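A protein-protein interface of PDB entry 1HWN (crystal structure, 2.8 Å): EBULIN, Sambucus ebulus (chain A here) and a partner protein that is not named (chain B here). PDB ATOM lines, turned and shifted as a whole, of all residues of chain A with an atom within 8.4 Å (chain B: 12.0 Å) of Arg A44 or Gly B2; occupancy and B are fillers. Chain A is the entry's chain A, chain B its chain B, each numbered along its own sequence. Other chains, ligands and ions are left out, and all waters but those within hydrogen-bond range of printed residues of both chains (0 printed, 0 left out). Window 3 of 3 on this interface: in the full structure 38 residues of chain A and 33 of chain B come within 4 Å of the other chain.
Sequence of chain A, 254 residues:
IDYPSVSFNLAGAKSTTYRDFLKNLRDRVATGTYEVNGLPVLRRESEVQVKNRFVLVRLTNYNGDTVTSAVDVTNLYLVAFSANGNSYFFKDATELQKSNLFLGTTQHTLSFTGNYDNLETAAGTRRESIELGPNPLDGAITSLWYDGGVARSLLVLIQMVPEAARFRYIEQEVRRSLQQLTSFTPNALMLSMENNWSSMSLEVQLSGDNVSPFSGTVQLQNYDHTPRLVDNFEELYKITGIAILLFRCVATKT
The side-chain sulfur of Cys A249 sits close to the backbone carbonyl oxygen of Thr B4 (3.4 Å).
SG of Cys A249 sits close to O of Glu B3, at 3.1 Å.
The side-chain sulfur of Cys B5 sits close to the backbone carbonyl oxygen of Gln A205 (3.5 Å).
The backbone NH (N) of Val A250 sits at hydrogen-bond distance from the backbone carbonyl oxygen (O) of Glu B3, at 3.2 Å.
N of Cys B5 sits at hydrogen-bond distance from O of Val A250, at 3.3 Å.
SG of Cys A249 forms a disulfide with SG of Cys B5, at 2.0 Å.
Tyr A34 touches none of the printed residues of chain B.
Arg A44 touches just one residue of chain B: Gly B2 (3.5 Å).
No residue of chain B comes within 4 Å of Glu A45.
No residue of chain B comes within 4 Å of Ser A46.
No residue of chain B comes within 4 Å of Glu A47.
No residue of chain B comes within 4 Å of Val A48.
Thr A74 touches none of the printed residues of chain B.
Printed residues of chain B within 4 Å of Gln A205: Cys B5 (3.5 Å).
No residue of chain B comes within 4 Å of Phe A247.
Cys A249 touches just these residues of chain B: Glu B3, Thr B4 and Cys B5.
Gly B2 touches just one residue of chain A: Arg A44.
Printed residues of chain A within 4 Å of Glu B3: Cys A249 (3.1 Å) and Val A250 (3.2 Å).
Of the printed residues of chain A, Cys B5 touches Gln A205, Cys A249 and Val A250.
Ala B6 touches none of the printed residues of chain A.
The nearest printed residue of chain B that does not touch Gln A205 is Thr B4 (7.5 Å).
Of the 22 printed residues of chain A, 4 touch a printed residue of chain B.
Printed residues of chain A that touch a printed residue of chain B: Arg A44, Gln A205, Cys A249 and Val A250.
Hydrophobic or aromatic side chains of chain A that line the printed part of chain B: Val A250.
Among the printed residues, 8 pairs touch across the chains.
Among the printed residues, no Asp or Glu carboxylate lies within 4 Å of a Lys or Arg side-chain nitrogen of the other chain.
Among the printed residues, merely in contact across the chains: Arg A44 with Gly B2 and Val A250 with Thr B4.
OG of Ser A46 sits close to NE of Arg A44 (3.2 Å).
The backbone NH (N) of Arg A248 lies close to the side-chain amide nitrogen (NE2) of Gln A205 (3.1 Å).
The side-chain amide nitrogen (NE2) of Gln A205 lies within hydrogen-bond range of the backbone carbonyl oxygen (O) of Leu A246 (3.3 Å).
The side-chain amide oxygen (OE1) of Gln A205 sits close to the backbone carbonyl oxygen (O) of Cys A249 (2.7 Å).
The backbone carbonyl oxygen of Cys A249 lies within hydrogen-bond range of the side-chain hydroxyl of Tyr A34 (3.0 Å).
The side-chain amide oxygen (OE1) of Gln A205 is in hydrogen-bond range of the side-chain hydroxyl (OH) of Tyr A34 (3.2 Å).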
ATOM      1  N   THR A  31     -31.903  16.707  20.189  1.00  0.00           N
ATOM      2  CA  THR A  31     -33.062  17.169  19.436  1.00  0.00           C
ATOM      3  C   THR A  31     -32.623  18.044  18.267  1.00  0.00           C
ATOM      4  O   THR A  31     -32.162  19.171  18.454  1.00  0.00           O
ATOM      5  CB  THR A  31     -34.036  17.975  20.333  1.00  0.00           C
ATOM      6  OG1 THR A  31     -33.496  19.278  20.588  1.00  0.00           O
ATOM      7  CG2 THR A  31     -34.263  17.255  21.654  1.00  0.00           C
ATOM      8  N   TYR A  34     -30.618  16.580  11.866  1.00  0.00           N
ATOM      9  CA  TYR A  34     -29.336  16.385  11.200  1.00  0.00           C
ATOM     10  C   TYR A  34     -28.609  15.189  11.803  1.00  0.00           C
ATOM     11  O   TYR A  34     -28.139  15.243  12.941  1.00  0.00           O
ATOM     12  CB  TYR A  34     -28.474  17.644  11.337  1.00  0.00           C
ATOM     13  CG  TYR A  34     -27.173  17.613  10.558  1.00  0.00           C
ATOM     14  CD1 TYR A  34     -26.197  18.586  10.764  1.00  0.00           C
ATOM     15  CD2 TYR A  34     -26.916  16.612   9.618  1.00  0.00           C
ATOM     16  CE1 TYR A  34     -24.998  18.566  10.057  1.00  0.00           C
ATOM     17  CE2 TYR A  34     -25.720  16.585   8.906  1.00  0.00           C
ATOM     18  CZ  TYR A  34     -24.766  17.565   9.131  1.00  0.00           C
ATOM     19  OH  TYR A  34     -23.581  17.545   8.432  1.00  0.00           O
ATOM     20  N   VAL A  41     -25.822  15.618  14.961  1.00  0.00           N
ATOM     21  CA  VAL A  41     -24.933  16.769  14.866  1.00  0.00           C
ATOM     22  C   VAL A  41     -25.553  17.957  15.599  1.00  0.00           C
ATOM     23  O   VAL A  41     -26.382  18.675  15.040  1.00  0.00           O
ATOM     24  CB  VAL A  41     -24.693  17.168  13.392  1.00  0.00           C
ATOM     25  CG1 VAL A  41     -23.658  18.277  13.319  1.00  0.00           C
ATOM     26  CG2 VAL A  41     -24.236  15.961  12.589  1.00  0.00           C
ATOM     27  N   LEU A  42     -25.149  18.150  16.851  1.00  0.00           N
ATOM     28  CA  LEU A  42     -25.660  19.243  17.675  1.00  0.00           C
ATOM     29  C   LEU A  42     -25.876  20.525  16.878  1.00  0.00           C
ATOM     30  O   LEU A  42     -25.057  20.887  16.030  1.00  0.00           O
ATOM     31  CB  LEU A  42     -24.699  19.523  18.835  1.00  0.00           C
ATOM     32  CG  LEU A  42     -24.161  18.322  19.617  1.00  0.00           C
ATOM     33  CD1 LEU A  42     -23.221  18.814  20.705  1.00  0.00           C
ATOM     34  CD2 LEU A  42     -25.311  17.529  20.220  1.00  0.00           C
ATOM     35  N   ARG A  43     -26.981  21.208  17.157  1.00  0.00           N
ATOM     36  CA  ARG A  43     -27.311  22.451  16.468  1.00  0.00           C
ATOM     37  C   ARG A  43     -26.265  23.525  16.743  1.00  0.00           C
ATOM     38  O   ARG A  43     -25.440  23.381  17.646  1.00  0.00           O
ATOM     39  CB  ARG A  43     -28.685  22.952  16.916  1.00  0.00           C
ATOM     40  CG  ARG A  43     -29.707  21.849  17.122  1.00  0.00           C
ATOM     41  CD  ARG A  43     -30.686  22.205  18.227  1.00  0.00           C
ATOM     42  NE  ARG A  43     -30.701  21.200  19.286  1.00  0.00           N
ATOM     43  CZ  ARG A  43     -31.032  21.450  20.548  1.00  0.00           C
ATOM     44  NH1 ARG A  43     -31.379  22.678  20.913  1.00  0.00           N
ATOM     45  NH2 ARG A  43     -31.017  20.474  21.444  1.00  0.00           N
ATOM     46  N   ARG A  44     -26.309  24.601  15.966  1.00  0.00           N
ATOM     47  CA  ARG A  44     -25.364  25.700  16.131  1.00  0.00           C
ATOM     48  C   ARG A  44     -26.052  26.933  16.706  1.00  0.00           C
ATOM     49  O   ARG A  44     -27.282  27.012  16.739  1.00  0.00           O
ATOM     50  CB  ARG A  44     -24.712  26.054  14.788  1.00  0.00           C
ATOM     51  CG  ARG A  44     -25.477  25.567  13.567  1.00  0.00           C
ATOM     52  CD  ARG A  44     -25.712  26.700  12.580  1.00  0.00           C
ATOM     53  NE  ARG A  44     -24.555  26.917  11.716  1.00  0.00           N
ATOM     54  CZ  ARG A  44     -24.430  26.408  10.495  1.00  0.00           C
ATOM     55  NH1 ARG A  44     -25.392  25.649   9.987  1.00  0.00           N
ATOM     56  NH2 ARG A  44     -23.340  26.659   9.780  1.00  0.00           N
ATOM     57  N   GLU A  45     -25.250  27.892  17.154  1.00  0.00           N
ATOM     58  CA  GLU A  45     -25.776  29.123  17.734  1.00  0.00           C
ATOM     59  C   GLU A  45     -26.657  29.860  16.733  1.00  0.00           C
ATOM     60  O   GLU A  45     -27.651  30.484  17.105  1.00  0.00           O
ATOM     61  CB  GLU A  45     -24.626  30.033  18.178  1.00  0.00           C
ATOM     62  CG  GLU A  45     -23.400  29.286  18.695  1.00  0.00           C
ATOM     63  CD  GLU A  45     -22.291  30.219  19.158  1.00  0.00           C
ATOM     64  OE1 GLU A  45     -22.559  31.428  19.335  1.00  0.00           O
ATOM     65  OE2 GLU A  45     -21.152  29.740  19.343  1.00  0.00           O
ATOM     66  N   SER A  46     -26.287  29.774  15.460  1.00  0.00           N
ATOM     67  CA  SER A  46     -27.026  30.433  14.389  1.00  0.00           C
ATOM     68  C   SER A  46     -28.501  30.044  14.362  1.00  0.00           C
ATOM     69  O   SER A  46     -29.336  30.793  13.859  1.00  0.00           O
ATOM     70  CB  SER A  46     -26.389  30.105  13.037  1.00  0.00           C
ATOM     71  OG  SER A  46     -25.036  29.706  13.194  1.00  0.00           O
ATOM     72  N   GLU A  47     -28.820  28.873  14.904  1.00  0.00           N
ATOM     73  CA  GLU A  47     -30.201  28.407  14.924  1.00  0.00           C
ATOM     74  C   GLU A  47     -30.621  27.825  16.271  1.00  0.00           C
ATOM     75  O   GLU A  47     -31.340  26.827  16.328  1.00  0.00           O
ATOM     76  CB  GLU A  47     -30.417  27.363  13.825  1.00  0.00           C
ATOM     77  CG  GLU A  47     -29.200  26.496  13.538  1.00  0.00           C
ATOM     78  CD  GLU A  47     -29.507  25.015  13.645  1.00  0.00           C
ATOM     79  OE1 GLU A  47     -30.622  24.670  14.093  1.00  0.00           O
ATOM     80  OE2 GLU A  47     -28.636  24.196  13.281  1.00  0.00           O
ATOM     81  N   VAL A  48     -30.170  28.454  17.354  1.00  0.00           N
ATOM     82  CA  VAL A  48     -30.515  28.000  18.699  1.00  0.00           C
ATOM     83  C   VAL A  48     -31.199  29.114  19.489  1.00  0.00           C
ATOM     84  O   VAL A  48     -30.630  30.189  19.691  1.00  0.00           O
ATOM     85  CB  VAL A  48     -29.259  27.523  19.471  1.00  0.00           C
ATOM     86  CG1 VAL A  48     -28.297  28.680  19.677  1.00  0.00           C
ATOM     87  CG2 VAL A  48     -29.665  26.926  20.807  1.00  0.00           C
ATOM     88  N   GLN A  49     -32.427  28.857  19.927  1.00  0.00           N
ATOM     89  CA  GLN A  49     -33.180  29.847  20.689  1.00  0.00           C
ATOM     90  C   GLN A  49     -32.535  30.127  22.041  1.00  0.00           C
ATOM     91  O   GLN A  49     -31.859  29.271  22.609  1.00  0.00           O
ATOM     92  CB  GLN A  49     -34.622  29.375  20.900  1.00  0.00           C
ATOM     93  CG  GLN A  49     -35.650  30.499  20.858  1.00  0.00           C
ATOM     94  CD  GLN A  49     -35.690  31.198  19.512  1.00  0.00           C
ATOM     95  OE1 GLN A  49     -35.200  30.672  18.514  1.00  0.00           O
ATOM     96  NE2 GLN A  49     -36.273  32.392  19.478  1.00  0.00           N
ATOM     97  N   ARG A  53     -31.001  27.232  24.337  1.00  0.00           N
ATOM     98  CA  ARG A  53     -29.551  27.212  24.218  1.00  0.00           C
ATOM     99  C   ARG A  53     -28.853  26.343  25.257  1.00  0.00           C
ATOM    100  O   ARG A  53     -27.962  25.567  24.919  1.00  0.00           O
ATOM    101  CB  ARG A  53     -28.997  28.637  24.301  1.00  0.00           C
ATOM    102  CG  ARG A  53     -27.786  28.888  23.414  1.00  0.00           C
ATOM    103  CD  ARG A  53     -26.526  28.268  24.001  1.00  0.00           C
ATOM    104  NE  ARG A  53     -25.376  28.397  23.106  1.00  0.00           N
ATOM    105  CZ  ARG A  53     -24.885  29.555  22.679  1.00  0.00           C
ATOM    106  NH1 ARG A  53     -25.444  30.694  23.063  1.00  0.00           N
ATOM    107  NH2 ARG A  53     -23.834  29.575  21.873  1.00  0.00           N
ATOM    108  N   ASP A  72     -23.852  23.846  27.302  1.00  0.00           N
ATOM    109  CA  ASP A  72     -24.259  24.399  26.016  1.00  0.00           C
ATOM    110  C   ASP A  72     -24.836  23.303  25.125  1.00  0.00           C
ATOM    111  O   ASP A  72     -24.215  22.257  24.934  1.00  0.00           O
ATOM    112  CB  ASP A  72     -23.059  25.052  25.326  1.00  0.00           C
ATOM    113  CG  ASP A  72     -23.470  26.056  24.270  1.00  0.00           C
ATOM    114  OD1 ASP A  72     -24.570  25.900  23.697  1.00  0.00           O
ATOM    115  OD2 ASP A  72     -22.693  26.999  24.012  1.00  0.00           O
ATOM    116  N   VAL A  73     -26.024  23.545  24.583  1.00  0.00           N
ATOM    117  CA  VAL A  73     -26.685  22.573  23.720  1.00  0.00           C
ATOM    118  C   VAL A  73     -26.021  22.511  22.345  1.00  0.00           C
ATOM    119  O   VAL A  73     -26.323  21.632  21.535  1.00  0.00           O
ATOM    120  CB  VAL A  73     -28.191  22.912  23.552  1.00  0.00           C
ATOM    121  CG1 VAL A  73     -28.424  23.674  22.253  1.00  0.00           C
ATOM    122  CG2 VAL A  73     -29.015  21.636  23.576  1.00  0.00           C
ATOM    123  N   THR A  74     -25.113  23.446  22.090  1.00  0.00           N
ATOM    124  CA  THR A  74     -24.414  23.495  20.815  1.00  0.00           C
ATOM    125  C   THR A  74     -23.129  22.671  20.815  1.00  0.00           C
ATOM    126  O   THR A  74     -22.940  21.812  19.956  1.00  0.00           O
ATOM    127  CB  THR A  74     -24.069  24.948  20.424  1.00  0.00           C
ATOM    128  OG1 THR A  74     -22.969  25.410  21.215  1.00  0.00           O
ATOM    129  CG2 THR A  74     -25.268  25.858  20.658  1.00  0.00           C
ATOM    130  N   ASN A  75     -22.249  22.924  21.780  1.00  0.00           N
ATOM    131  CA  ASN A  75     -20.982  22.196  21.854  1.00  0.00           C
ATOM    132  C   ASN A  75     -20.866  21.285  23.075  1.00  0.00           C
ATOM    133  O   ASN A  75     -19.860  20.597  23.248  1.00  0.00           O
ATOM    134  CB  ASN A  75     -19.807  23.178  21.841  1.00  0.00           C
ATOM    135  CG  ASN A  75     -20.012  24.347  22.779  1.00  0.00           C
ATOM    136  OD1 ASN A  75     -20.590  24.198  23.855  1.00  0.00           O
ATOM    137  ND2 ASN A  75     -19.534  25.520  22.378  1.00  0.00           N
ATOM    138  N   GLN A 205     -18.612  14.179   9.061  1.00  0.00           N
ATOM    139  CA  GLN A 205     -19.510  14.983   8.245  1.00  0.00           C
ATOM    140  C   GLN A 205     -18.916  15.212   6.857  1.00  0.00           C
ATOM    141  O   GLN A 205     -19.641  15.446   5.892  1.00  0.00           O
ATOM    142  CB  GLN A 205     -19.785  16.325   8.931  1.00  0.00           C
ATOM    143  CG  GLN A 205     -20.649  16.205  10.180  1.00  0.00           C
ATOM    144  CD  GLN A 205     -20.711  17.493  10.976  1.00  0.00           C
ATOM    145  OE1 GLN A 205     -21.702  18.221  10.923  1.00  0.00           O
ATOM    146  NE2 GLN A 205     -19.650  17.782  11.718  1.00  0.00           N
ATOM    147  N   LEU A 246     -20.022  17.319  16.894  1.00  0.00           N
ATOM    148  CA  LEU A 246     -20.011  18.778  16.909  1.00  0.00           C
ATOM    149  C   LEU A 246     -20.044  19.324  15.485  1.00  0.00           C
ATOM    150  O   LEU A 246     -19.129  19.080  14.698  1.00  0.00           O
ATOM    151  CB  LEU A 246     -18.756  19.289  17.622  1.00  0.00           C
ATOM    152  CG  LEU A 246     -18.566  20.807  17.661  1.00  0.00           C
ATOM    153  CD1 LEU A 246     -19.641  21.427  18.538  1.00  0.00           C
ATOM    154  CD2 LEU A 246     -17.177  21.146  18.187  1.00  0.00           C
ATOM    155  N   PHE A 247     -21.096  20.067  15.154  1.00  0.00           N
ATOM    156  CA  PHE A 247     -21.223  20.625  13.814  1.00  0.00           C
ATOM    157  C   PHE A 247     -19.968  21.347  13.348  1.00  0.00           C
ATOM    158  O   PHE A 247     -19.594  22.387  13.891  1.00  0.00           O
ATOM    159  CB  PHE A 247     -22.407  21.591  13.732  1.00  0.00           C
ATOM    160  CG  PHE A 247     -22.667  22.102  12.339  1.00  0.00           C
ATOM    161  CD1 PHE A 247     -23.293  21.289  11.395  1.00  0.00           C
ATOM    162  CD2 PHE A 247     -22.262  23.377  11.960  1.00  0.00           C
ATOM    163  CE1 PHE A 247     -23.507  21.738  10.096  1.00  0.00           C
ATOM    164  CE2 PHE A 247     -22.473  23.837  10.661  1.00  0.00           C
ATOM    165  CZ  PHE A 247     -23.095  23.014   9.727  1.00  0.00           C
ATOM    166  N   ARG A 248     -19.325  20.785  12.330  1.00  0.00           N
ATOM    167  CA  ARG A 248     -18.121  21.372  11.762  1.00  0.00           C
ATOM    168  C   ARG A 248     -18.390  21.712  10.299  1.00  0.00           C
ATOM    169  O   ARG A 248     -17.654  22.483   9.683  1.00  0.00           O
ATOM    170  CB  ARG A 248     -16.952  20.386  11.854  1.00  0.00           C
ATOM    171  CG  ARG A 248     -16.273  20.340  13.213  1.00  0.00           C
ATOM    172  CD  ARG A 248     -15.571  21.650  13.536  1.00  0.00           C
ATOM    173  NE  ARG A 248     -14.754  22.133  12.427  1.00  0.00           N
ATOM    174  CZ  ARG A 248     -13.475  21.818  12.247  1.00  0.00           C
ATOM    175  NH1 ARG A 248     -12.859  21.015  13.104  1.00  0.00           N
ATOM    176  NH2 ARG A 248     -12.806  22.311  11.213  1.00  0.00           N
ATOM    177  N   CYS A 249     -19.462  21.138   9.756  1.00  0.00           N
ATOM    178  CA  CYS A 249     -19.834  21.358   8.365  1.00  0.00           C
ATOM    179  C   CYS A 249     -21.094  20.585   7.987  1.00  0.00           C
ATOM    180  O   CYS A 249     -21.509  19.664   8.693  1.00  0.00           O
ATOM    181  CB  CYS A 249     -18.689  20.928   7.445  1.00  0.00           C
ATOM    182  SG  CYS A 249     -19.180  20.738   5.704  1.00  0.00           S
ATOM    183  N   VAL A 250     -21.697  20.964   6.864  1.00  0.00           N
ATOM    184  CA  VAL A 250     -22.903  20.310   6.371  1.00  0.00           C
ATOM    185  C   VAL A 250     -22.559  19.428   5.168  1.00  0.00           C
ATOM    186  O   VAL A 250     -21.606  19.702   4.436  1.00  0.00           O
ATOM    187  CB  VAL A 250     -23.966  21.353   5.948  1.00  0.00           C
ATOM    188  CG1 VAL A 250     -23.400  22.269   4.877  1.00  0.00           C
ATOM    189  CG2 VAL A 250     -25.216  20.650   5.447  1.00  0.00           C
ATOM    190  N   GLY B   2     -24.732  28.529   5.983  1.00  0.00           N
ATOM    191  CA  GLY B   2     -23.939  27.358   6.455  1.00  0.00           C
ATOM    192  C   GLY B   2     -22.570  27.290   5.806  1.00  0.00           C
ATOM    193  O   GLY B   2     -21.961  28.321   5.518  1.00  0.00           O
ATOM    194  N   GLU B   3     -22.084  26.074   5.576  1.00  0.00           N
ATOM    195  CA  GLU B   3     -20.781  25.872   4.953  1.00  0.00           C
ATOM    196  C   GLU B   3     -20.613  24.425   4.501  1.00  0.00           C
ATOM    197  O   GLU B   3     -20.429  23.526   5.322  1.00  0.00           O
ATOM    198  CB  GLU B   3     -19.662  26.236   5.936  1.00  0.00           C
ATOM    199  CG  GLU B   3     -18.296  26.414   5.284  1.00  0.00           C
ATOM    200  CD  GLU B   3     -17.155  26.347   6.285  1.00  0.00           C
ATOM    201  OE1 GLU B   3     -16.716  25.226   6.616  1.00  0.00           O
ATOM    202  OE2 GLU B   3     -16.695  27.418   6.735  1.00  0.00           O
ATOM    203  N   THR B   4     -20.686  24.206   3.191  1.00  0.00           N
ATOM    204  CA  THR B   4     -20.534  22.866   2.635  1.00  0.00           C
ATOM    205  C   THR B   4     -19.153  22.324   2.999  1.00  0.00           C
ATOM    206  O   THR B   4     -18.268  23.081   3.402  1.00  0.00           O
ATOM    207  CB  THR B   4     -20.695  22.870   1.093  1.00  0.00           C
ATOM    208  OG1 THR B   4     -21.200  21.599   0.660  1.00  0.00           O
ATOM    209  CG2 THR B   4     -19.358  23.143   0.408  1.00  0.00           C
ATOM    210  N   CYS B   5     -18.973  21.015   2.857  1.00  0.00           N
ATOM    211  CA  CYS B   5     -17.701  20.384   3.189  1.00  0.00           C
ATOM    212  C   CYS B   5     -16.707  20.425   2.038  1.00  0.00           C
ATOM    213  O   CYS B   5     -17.056  20.158   0.889  1.00  0.00           O
ATOM    214  CB  CYS B   5     -17.932  18.937   3.631  1.00  0.00           C
ATOM    215  SG  CYS B   5     -18.727  18.808   5.264  1.00  0.00           S
ATOM    216  N   ALA B   6     -15.465  20.768   2.360  1.00  0.00           N
ATOM    217  CA  ALA B   6     -14.408  20.850   1.361  1.00  0.00           C
ATOM    218  C   ALA B   6     -14.255  19.525   0.628  1.00  0.00           C
ATOM    219  O   ALA B   6     -13.954  18.498   1.238  1.00  0.00           O
ATOM    220  CB  ALA B   6     -13.091  21.239   2.023  1.00  0.00           C
